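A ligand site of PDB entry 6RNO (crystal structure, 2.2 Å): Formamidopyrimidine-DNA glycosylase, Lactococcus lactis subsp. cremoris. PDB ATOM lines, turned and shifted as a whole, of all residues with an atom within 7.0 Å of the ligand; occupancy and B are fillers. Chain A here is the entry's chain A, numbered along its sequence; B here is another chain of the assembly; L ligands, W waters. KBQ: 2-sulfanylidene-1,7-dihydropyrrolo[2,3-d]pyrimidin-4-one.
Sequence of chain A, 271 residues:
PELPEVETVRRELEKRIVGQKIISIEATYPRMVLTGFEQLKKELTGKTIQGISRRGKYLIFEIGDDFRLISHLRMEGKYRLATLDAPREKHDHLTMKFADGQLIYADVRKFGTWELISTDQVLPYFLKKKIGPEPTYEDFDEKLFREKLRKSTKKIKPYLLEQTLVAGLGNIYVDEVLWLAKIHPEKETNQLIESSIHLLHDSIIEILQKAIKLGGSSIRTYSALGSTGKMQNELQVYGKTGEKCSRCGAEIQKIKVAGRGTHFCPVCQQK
OP2 of DT 9 of chain B lies within hydrogen-bond range of a nitrogen (N3) of the ligand (2.6 Å).
A nitrogen (N3) of the ligand sits at hydrogen-bond distance from the backbone carbonyl oxygen (O) of Leu 161, 3.0 Å away.
A sulfur (S2) of the ligand sits close to the guanidinium group (NH1) of Arg 260, 3.5 Å away.
The side-chain amino group (NZ) of Lys 57 sits close to a sulfur (S2) of the ligand, at 3.6 Å.
OP2 of DT 9 of chain B is in salt-bridge range of NZ of Lys 57, 2.8 Å away.
NE2 of Gln 163 sits at hydrogen-bond distance from O of Leu 161, at 3.0 Å.
The guanidinium group (NH2) of Arg 260 is in salt-bridge range of OP2 of DT 8 of chain B, at 2.9 Å.
OP2 of 3DR 7 of chain B is in salt-bridge range of NH2 of Arg 260 (3.0 Å).
NZ of Lys 57 lies within salt-bridge range of OP1 of DT 8 of chain B, at 2.7 Å.
NZ of Lys 57 sits close to NE2 of Gln 163 (3.4 Å).
O of Leu 169 lies within hydrogen-bond range of NZ of Lys 57, at 2.8 Å.
The side-chain amide nitrogen (NE2) of Gln 163 lies within hydrogen-bond range of the backbone carbonyl oxygen (O) of Leu 169 (2.8 Å).
OP2 of DT 8 of chain B lies close to a sulfur (S2) of the ligand, at 3.6 Å.
Glu 162 touches the ligand (O to C8, 3.7 Å).
Gln 163 touches the ligand (CG to N9, 3.8 Å).
DT 10 of chain B touches the ligand (C7 to C7, 3.4 Å).
Hydrophobic or aromatic side chains within 4 Å of the ligand: Leu 161.
Within 4 Å of the ligand: Lys 57, Leu 161, Glu 162, Gln 163, Arg 260, DT 8 of chain B, DT 9 of chain B and DT 10 of chain B.
Water W1 bridges O6 of the ligand (2.6 Å) and O of Pro 158 (2.9 Å).
Water W4 bridges a nitrogen (N1) of the ligand (3.0 Å) and the guanidinium group (NH1) of Arg 260 (3.1 Å).
Water W3 lies within hydrogen-bond range of the side-chain hydroxyl (OH) of Tyr 58, O5' of DT 9 of chain B and a nitrogen (N9) of the ligand.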
ATOM      1  N   LYS A  57       2.442  -2.875 -16.600  1.00  0.00           N
ATOM      2  CA  LYS A  57       2.091  -3.156 -18.001  1.00  0.00           C
ATOM      3  C   LYS A  57       3.309  -3.562 -18.871  1.00  0.00           C
ATOM      4  O   LYS A  57       3.201  -3.657 -20.097  1.00  0.00           O
ATOM      5  CB  LYS A  57       1.424  -1.910 -18.607  1.00  0.00           C
ATOM      6  CG  LYS A  57       0.210  -1.464 -17.801  1.00  0.00           C
ATOM      7  CD  LYS A  57      -0.358  -0.153 -18.325  1.00  0.00           C
ATOM      8  CE  LYS A  57      -1.179   0.498 -17.227  1.00  0.00           C
ATOM      9  NZ  LYS A  57      -1.581   1.873 -17.568  1.00  0.00           N
ATOM     10  N   TYR A  58       4.456  -3.759 -18.234  1.00  0.00           N
ATOM     11  CA  TYR A  58       5.700  -4.078 -18.949  1.00  0.00           C
ATOM     12  C   TYR A  58       5.934  -5.584 -19.082  1.00  0.00           C
ATOM     13  O   TYR A  58       5.891  -6.348 -18.101  1.00  0.00           O
ATOM     14  CB  TYR A  58       6.923  -3.469 -18.244  1.00  0.00           C
ATOM     15  CG  TYR A  58       6.911  -1.966 -18.128  1.00  0.00           C
ATOM     16  CD1 TYR A  58       6.026  -1.307 -17.284  1.00  0.00           C
ATOM     17  CD2 TYR A  58       7.813  -1.190 -18.868  1.00  0.00           C
ATOM     18  CE1 TYR A  58       6.046   0.089 -17.179  1.00  0.00           C
ATOM     19  CE2 TYR A  58       7.854   0.198 -18.766  1.00  0.00           C
ATOM     20  CZ  TYR A  58       6.973   0.818 -17.922  1.00  0.00           C
ATOM     21  OH  TYR A  58       7.010   2.184 -17.859  1.00  0.00           O
ATOM     22  N   LYS A 129      11.674   4.288 -12.454  1.00  0.00           N
ATOM     23  CA  LYS A 129      10.333   4.666 -12.903  1.00  0.00           C
ATOM     24  C   LYS A 129       9.361   4.826 -11.731  1.00  0.00           C
ATOM     25  O   LYS A 129       8.218   5.213 -11.918  1.00  0.00           O
ATOM     26  CB  LYS A 129       9.763   3.640 -13.853  1.00  0.00           C
ATOM     27  CG  LYS A 129      10.708   3.186 -14.918  1.00  0.00           C
ATOM     28  CD  LYS A 129      10.390   3.869 -16.210  1.00  0.00           C
ATOM     29  CE  LYS A 129      10.833   3.008 -17.337  1.00  0.00           C
ATOM     30  NZ  LYS A 129      11.454   3.875 -18.328  1.00  0.00           N
ATOM     31  N   ILE A 131       7.702   2.717 -10.294  1.00  0.00           N
ATOM     32  CA  ILE A 131       6.537   1.842 -10.439  1.00  0.00           C
ATOM     33  C   ILE A 131       6.078   1.263  -9.071  1.00  0.00           C
ATOM     34  O   ILE A 131       6.886   0.682  -8.363  1.00  0.00           O
ATOM     35  CB  ILE A 131       6.846   0.654 -11.389  1.00  0.00           C
ATOM     36  CG1 ILE A 131       7.228   1.141 -12.792  1.00  0.00           C
ATOM     37  CG2 ILE A 131       5.684  -0.290 -11.451  1.00  0.00           C
ATOM     38  CD1 ILE A 131       6.214   2.020 -13.477  1.00  0.00           C
ATOM     39  N   PRO A 158      -6.279  10.501 -12.068  1.00  0.00           N
ATOM     40  CA  PRO A 158      -4.937  10.670 -12.635  1.00  0.00           C
ATOM     41  C   PRO A 158      -3.820  10.131 -11.707  1.00  0.00           C
ATOM     42  O   PRO A 158      -2.811   9.625 -12.202  1.00  0.00           O
ATOM     43  CB  PRO A 158      -4.782  12.199 -12.782  1.00  0.00           C
ATOM     44  CG  PRO A 158      -6.121  12.749 -12.628  1.00  0.00           C
ATOM     45  CD  PRO A 158      -6.930  11.794 -11.836  1.00  0.00           C
ATOM     46  N   LEU A 160      -3.937   7.481  -9.656  1.00  0.00           N
ATOM     47  CA  LEU A 160      -3.893   6.041  -9.892  1.00  0.00           C
ATOM     48  C   LEU A 160      -3.248   5.695 -11.255  1.00  0.00           C
ATOM     49  O   LEU A 160      -2.541   4.694 -11.366  1.00  0.00           O
ATOM     50  CB  LEU A 160      -5.306   5.441  -9.803  1.00  0.00           C
ATOM     51  CG  LEU A 160      -5.970   5.382  -8.421  1.00  0.00           C
ATOM     52  CD1 LEU A 160      -7.430   4.933  -8.553  1.00  0.00           C
ATOM     53  CD2 LEU A 160      -5.218   4.455  -7.456  1.00  0.00           C
ATOM     54  N   LEU A 161      -3.493   6.513 -12.271  1.00  0.00           N
ATOM     55  CA  LEU A 161      -2.948   6.256 -13.611  1.00  0.00           C
ATOM     56  C   LEU A 161      -1.433   6.436 -13.650  1.00  0.00           C
ATOM     57  O   LEU A 161      -0.765   5.940 -14.575  1.00  0.00           O
ATOM     58  CB  LEU A 161      -3.628   7.170 -14.648  1.00  0.00           C
ATOM     59  CG  LEU A 161      -5.069   6.732 -14.957  1.00  0.00           C
ATOM     60  CD1 LEU A 161      -5.739   7.627 -16.005  1.00  0.00           C
ATOM     61  CD2 LEU A 161      -5.118   5.285 -15.441  1.00  0.00           C
ATOM     62  N   GLU A 162      -0.875   7.129 -12.654  1.00  0.00           N
ATOM     63  CA  GLU A 162       0.564   7.381 -12.663  1.00  0.00           C
ATOM     64  C   GLU A 162       1.435   6.134 -12.416  1.00  0.00           C
ATOM     65  O   GLU A 162       2.633   6.200 -12.651  1.00  0.00           O
ATOM     66  CB  GLU A 162       0.924   8.462 -11.649  1.00  0.00           C
ATOM     67  CG  GLU A 162       0.437   9.835 -12.067  1.00  0.00           C
ATOM     68  CD  GLU A 162       0.807  10.937 -11.096  1.00  0.00           C
ATOM     69  OE1 GLU A 162       1.523  10.671 -10.100  1.00  0.00           O
ATOM     70  OE2 GLU A 162       0.379  12.078 -11.342  1.00  0.00           O
ATOM     71  N   GLN A 163       0.830   5.007 -11.986  1.00  0.00           N
ATOM     72  CA  GLN A 163       1.509   3.714 -11.817  1.00  0.00           C
ATOM     73  C   GLN A 163       2.360   3.652 -10.547  1.00  0.00           C
ATOM     74  O   GLN A 163       3.062   2.656 -10.332  1.00  0.00           O
ATOM     75  CB  GLN A 163       2.415   3.384 -13.022  1.00  0.00           C
ATOM     76  CG  GLN A 163       1.722   3.343 -14.396  1.00  0.00           C
ATOM     77  CD  GLN A 163       0.559   2.390 -14.407  1.00  0.00           C
ATOM     78  OE1 GLN A 163       0.741   1.174 -14.339  1.00  0.00           O
ATOM     79  NE2 GLN A 163      -0.649   2.932 -14.448  1.00  0.00           N
ATOM     80  N   THR A 164       2.340   4.712  -9.733  1.00  0.00           N
ATOM     81  CA  THR A 164       3.222   4.784  -8.544  1.00  0.00           C
ATOM     82  C   THR A 164       2.527   4.376  -7.234  1.00  0.00           C
ATOM     83  O   THR A 164       3.198   3.983  -6.297  1.00  0.00           O
ATOM     84  CB  THR A 164       3.798   6.201  -8.341  1.00  0.00           C
ATOM     85  OG1 THR A 164       2.715   7.126  -8.154  1.00  0.00           O
ATOM     86  CG2 THR A 164       4.640   6.638  -9.545  1.00  0.00           C
ATOM     87  N   LEU A 169      -3.044  -0.218 -13.628  1.00  0.00           N
ATOM     88  CA  LEU A 169      -4.316   0.371 -14.005  1.00  0.00           C
ATOM     89  C   LEU A 169      -4.147   1.279 -15.216  1.00  0.00           C
ATOM     90  O   LEU A 169      -3.202   2.062 -15.283  1.00  0.00           O
ATOM     91  CB  LEU A 169      -4.934   1.160 -12.876  1.00  0.00           C
ATOM     92  CG  LEU A 169      -5.413   0.396 -11.640  1.00  0.00           C
ATOM     93  CD1 LEU A 169      -5.554   1.396 -10.508  1.00  0.00           C
ATOM     94  CD2 LEU A 169      -6.728  -0.329 -11.898  1.00  0.00           C
ATOM     95  N   GLY A 170      -5.054   1.168 -16.165  1.00  0.00           N
ATOM     96  CA  GLY A 170      -5.175   2.152 -17.228  1.00  0.00           C
ATOM     97  C   GLY A 170      -6.606   2.656 -17.280  1.00  0.00           C
ATOM     98  O   GLY A 170      -7.380   2.444 -16.350  1.00  0.00           O
ATOM     99  N   ASN A 171      -6.968   3.307 -18.381  1.00  0.00           N
ATOM    100  CA  ASN A 171      -8.205   4.058 -18.436  1.00  0.00           C
ATOM    101  C   ASN A 171      -9.427   3.192 -18.196  1.00  0.00           C
ATOM    102  O   ASN A 171     -10.333   3.605 -17.471  1.00  0.00           O
ATOM    103  CB  ASN A 171      -8.331   4.784 -19.772  1.00  0.00           C
ATOM    104  CG  ASN A 171      -9.089   6.083 -19.624  1.00  0.00           C
ATOM    105  OD1 ASN A 171      -9.074   6.658 -18.542  1.00  0.00           O
ATOM    106  ND2 ASN A 171      -9.754   6.575 -20.698  1.00  0.00           N
ATOM    107  N   ALA A 258      -8.076  15.296 -16.559  1.00  0.00           N
ATOM    108  CA  ALA A 258      -6.630  15.374 -16.775  1.00  0.00           C
ATOM    109  C   ALA A 258      -6.282  14.699 -18.076  1.00  0.00           C
ATOM    110  O   ALA A 258      -5.398  13.842 -18.130  1.00  0.00           O
ATOM    111  CB  ALA A 258      -5.874  14.733 -15.639  1.00  0.00           C
ATOM    112  N   ARG A 260      -7.993  12.546 -19.927  1.00  0.00           N
ATOM    113  CA  ARG A 260      -8.506  11.225 -20.286  1.00  0.00           C
ATOM    114  C   ARG A 260     -10.030  11.213 -20.354  1.00  0.00           C
ATOM    115  O   ARG A 260     -10.698  11.879 -19.547  1.00  0.00           O
ATOM    116  CB  ARG A 260      -8.023  10.164 -19.312  1.00  0.00           C
ATOM    117  CG  ARG A 260      -6.488  10.109 -19.101  1.00  0.00           C
ATOM    118  CD  ARG A 260      -5.739   9.848 -20.394  1.00  0.00           C
ATOM    119  NE  ARG A 260      -6.077   8.584 -21.060  1.00  0.00           N
ATOM    120  CZ  ARG A 260      -5.507   7.411 -20.785  1.00  0.00           C
ATOM    121  NH1 ARG A 260      -4.584   7.322 -19.831  1.00  0.00           N
ATOM    122  NH2 ARG A 260      -5.868   6.315 -21.464  1.00  0.00           N
ATOM    123  O5' 3DR B   7      -7.547   4.115 -23.338  1.00  0.00           O
ATOM    124  P   3DR B   7      -8.534   5.222 -23.824  1.00  0.00           P
ATOM    125  OP1 3DR B   7      -9.849   5.139 -23.153  1.00  0.00           O
ATOM    126  OP2 3DR B   7      -7.900   6.585 -23.679  1.00  0.00           O
ATOM    127  C2' 3DR B   7      -5.127   1.237 -23.746  1.00  0.00           C
ATOM    128  C5' 3DR B   7      -7.743   2.757 -23.486  1.00  0.00           C
ATOM    129  C4' 3DR B   7      -6.911   1.920 -22.579  1.00  0.00           C
ATOM    130  O4' 3DR B   7      -7.144   0.576 -22.812  1.00  0.00           O
ATOM    131  C1' 3DR B   7      -6.000   0.064 -23.421  1.00  0.00           C
ATOM    132  C3' 3DR B   7      -5.448   2.152 -22.763  1.00  0.00           C
ATOM    133  O3' 3DR B   7      -4.762   1.734 -21.635  1.00  0.00           O
ATOM    134  P    DT B   8      -3.850   2.751 -20.782  1.00  0.00           P
ATOM    135  OP1  DT B   8      -3.255   1.927 -19.704  1.00  0.00           O
ATOM    136  OP2  DT B   8      -4.614   3.941 -20.395  1.00  0.00           O
ATOM    137  O5'  DT B   8      -2.706   3.219 -21.815  1.00  0.00           O
ATOM    138  C5'  DT B   8      -1.839   2.270 -22.381  1.00  0.00           C
ATOM    139  C4'  DT B   8      -0.388   2.639 -22.122  1.00  0.00           C
ATOM    140  O4'  DT B   8       0.049   3.604 -23.105  1.00  0.00           O
ATOM    141  C3'  DT B   8      -0.064   3.218 -20.727  1.00  0.00           C
ATOM    142  O3'  DT B   8       1.169   2.606 -20.241  1.00  0.00           O
ATOM    143  C2'  DT B   8       0.073   4.723 -20.991  1.00  0.00           C
ATOM    144  C1'  DT B   8       0.506   4.782 -22.467  1.00  0.00           C
ATOM    145  N1   DT B   8      -0.055   5.917 -23.248  1.00  0.00           N
ATOM    146  C2   DT B   8       0.746   6.566 -24.180  1.00  0.00           C
ATOM    147  O2   DT B   8       1.903   6.265 -24.383  1.00  0.00           O
ATOM    148  N3   DT B   8       0.136   7.587 -24.857  1.00  0.00           N
ATOM    149  C4   DT B   8      -1.161   8.010 -24.726  1.00  0.00           C
ATOM    150  O4   DT B   8      -1.614   8.919 -25.396  1.00  0.00           O
ATOM    151  C5   DT B   8      -1.957   7.302 -23.743  1.00  0.00           C
ATOM    152  C7   DT B   8      -3.395   7.679 -23.516  1.00  0.00           C
ATOM    153  C6   DT B   8      -1.367   6.290 -23.062  1.00  0.00           C
ATOM    154  P    DT B   9       1.790   2.932 -18.785  1.00  0.00           P
ATOM    155  OP1  DT B   9       2.671   1.800 -18.393  1.00  0.00           O
ATOM    156  OP2  DT B   9       0.757   3.353 -17.836  1.00  0.00           O
ATOM    157  O5'  DT B   9       2.738   4.134 -19.124  1.00  0.00           O
ATOM    158  C5'  DT B   9       3.815   3.861 -20.005  1.00  0.00           C
ATOM    159  C4'  DT B   9       4.502   5.119 -20.463  1.00  0.00           C
ATOM    160  O4'  DT B   9       3.595   5.959 -21.206  1.00  0.00           O
ATOM    161  C3'  DT B   9       5.109   5.981 -19.351  1.00  0.00           C
ATOM    162  O3'  DT B   9       6.521   5.834 -19.511  1.00  0.00           O
ATOM    163  C2'  DT B   9       4.574   7.420 -19.651  1.00  0.00           C
ATOM    164  C1'  DT B   9       4.045   7.288 -21.089  1.00  0.00           C
ATOM    165  N1   DT B   9       2.898   8.196 -21.459  1.00  0.00           N
ATOM    166  C2   DT B   9       3.026   9.040 -22.538  1.00  0.00           C
ATOM    167  O2   DT B   9       4.040   9.136 -23.169  1.00  0.00           O
ATOM    168  N3   DT B   9       1.922   9.772 -22.848  1.00  0.00           N
ATOM    169  C4   DT B   9       0.708   9.752 -22.196  1.00  0.00           C
ATOM    170  O4   DT B   9      -0.224  10.455 -22.533  1.00  0.00           O
ATOM    171  C5   DT B   9       0.616   8.832 -21.079  1.00  0.00           C
ATOM    172  C7   DT B   9      -0.650   8.717 -20.263  1.00  0.00           C
ATOM    173  C6   DT B   9       1.707   8.098 -20.788  1.00  0.00           C
ATOM    174  P    DT B  10       7.603   6.670 -18.691  1.00  0.00           P
ATOM    175  OP1  DT B  10       8.822   5.853 -18.844  1.00  0.00           O
ATOM    176  OP2  DT B  10       7.064   7.028 -17.356  1.00  0.00           O
ATOM    177  O5'  DT B  10       7.833   7.994 -19.552  1.00  0.00           O
ATOM    178  C5'  DT B  10       8.214   7.897 -20.901  1.00  0.00           C
ATOM    179  C4'  DT B  10       8.388   9.269 -21.522  1.00  0.00           C
ATOM    180  O4'  DT B  10       7.100   9.868 -21.805  1.00  0.00           O
ATOM    181  C3'  DT B  10       9.137  10.276 -20.672  1.00  0.00           C
ATOM    182  O3'  DT B  10      10.045  10.940 -21.510  1.00  0.00           O
ATOM    183  C2'  DT B  10       8.037  11.215 -20.158  1.00  0.00           C
ATOM    184  C1'  DT B  10       7.096  11.206 -21.349  1.00  0.00           C
ATOM    185  N1   DT B  10       5.672  11.577 -21.042  1.00  0.00           N
ATOM    186  C2   DT B  10       5.000  12.394 -21.925  1.00  0.00           C
ATOM    187  O2   DT B  10       5.517  12.855 -22.923  1.00  0.00           O
ATOM    188  N3   DT B  10       3.685  12.637 -21.612  1.00  0.00           N
ATOM    189  C4   DT B  10       2.992  12.155 -20.522  1.00  0.00           C
ATOM    190  O4   DT B  10       1.827  12.446 -20.317  1.00  0.00           O
ATOM    191  C5   DT B  10       3.744  11.298 -19.621  1.00  0.00           C
ATOM    192  C7   DT B  10       3.097  10.724 -18.394  1.00  0.00           C
ATOM    193  C6   DT B  10       5.040  11.053 -19.931  1.00  0.00           C
HETATM  194  N1  KBQ L   1      -1.132   7.712 -17.210  1.00  0.00           N
HETATM  195  N3  KBQ L   1       0.309   5.865 -17.341  1.00  0.00           N
HETATM  196  C4  KBQ L   1       1.325   6.607 -16.850  1.00  0.00           C
HETATM  197  C5  KBQ L   1       1.119   7.917 -16.521  1.00  0.00           C
HETATM  198  C6  KBQ L   1      -0.127   8.473 -16.709  1.00  0.00           C
HETATM  199  C7  KBQ L   1       2.305   8.408 -16.050  1.00  0.00           C
HETATM  200  C8  KBQ L   1       3.242   7.406 -16.077  1.00  0.00           C
HETATM  201  C2  KBQ L   1      -0.923   6.392 -17.529  1.00  0.00           C
HETATM  202  N9  KBQ L   1       2.627   6.302 -16.571  1.00  0.00           N
HETATM  203  O6  KBQ L   1      -0.326   9.652 -16.427  1.00  0.00           O
HETATM  204  S2  KBQ L   1      -2.148   5.410 -18.158  1.00  0.00           S
HETATM  205  O   HOH W   1      -2.254  10.475 -14.876  1.00  0.00           O
HETATM  206  O   HOH W   2       0.908  11.880 -15.513  1.00  0.00           O
HETATM  207  O   HOH W   3       4.577   3.602 -16.672  1.00  0.00           O
HETATM  208  O   HOH W   4      -3.332   9.496 -18.076  1.00  0.00           O
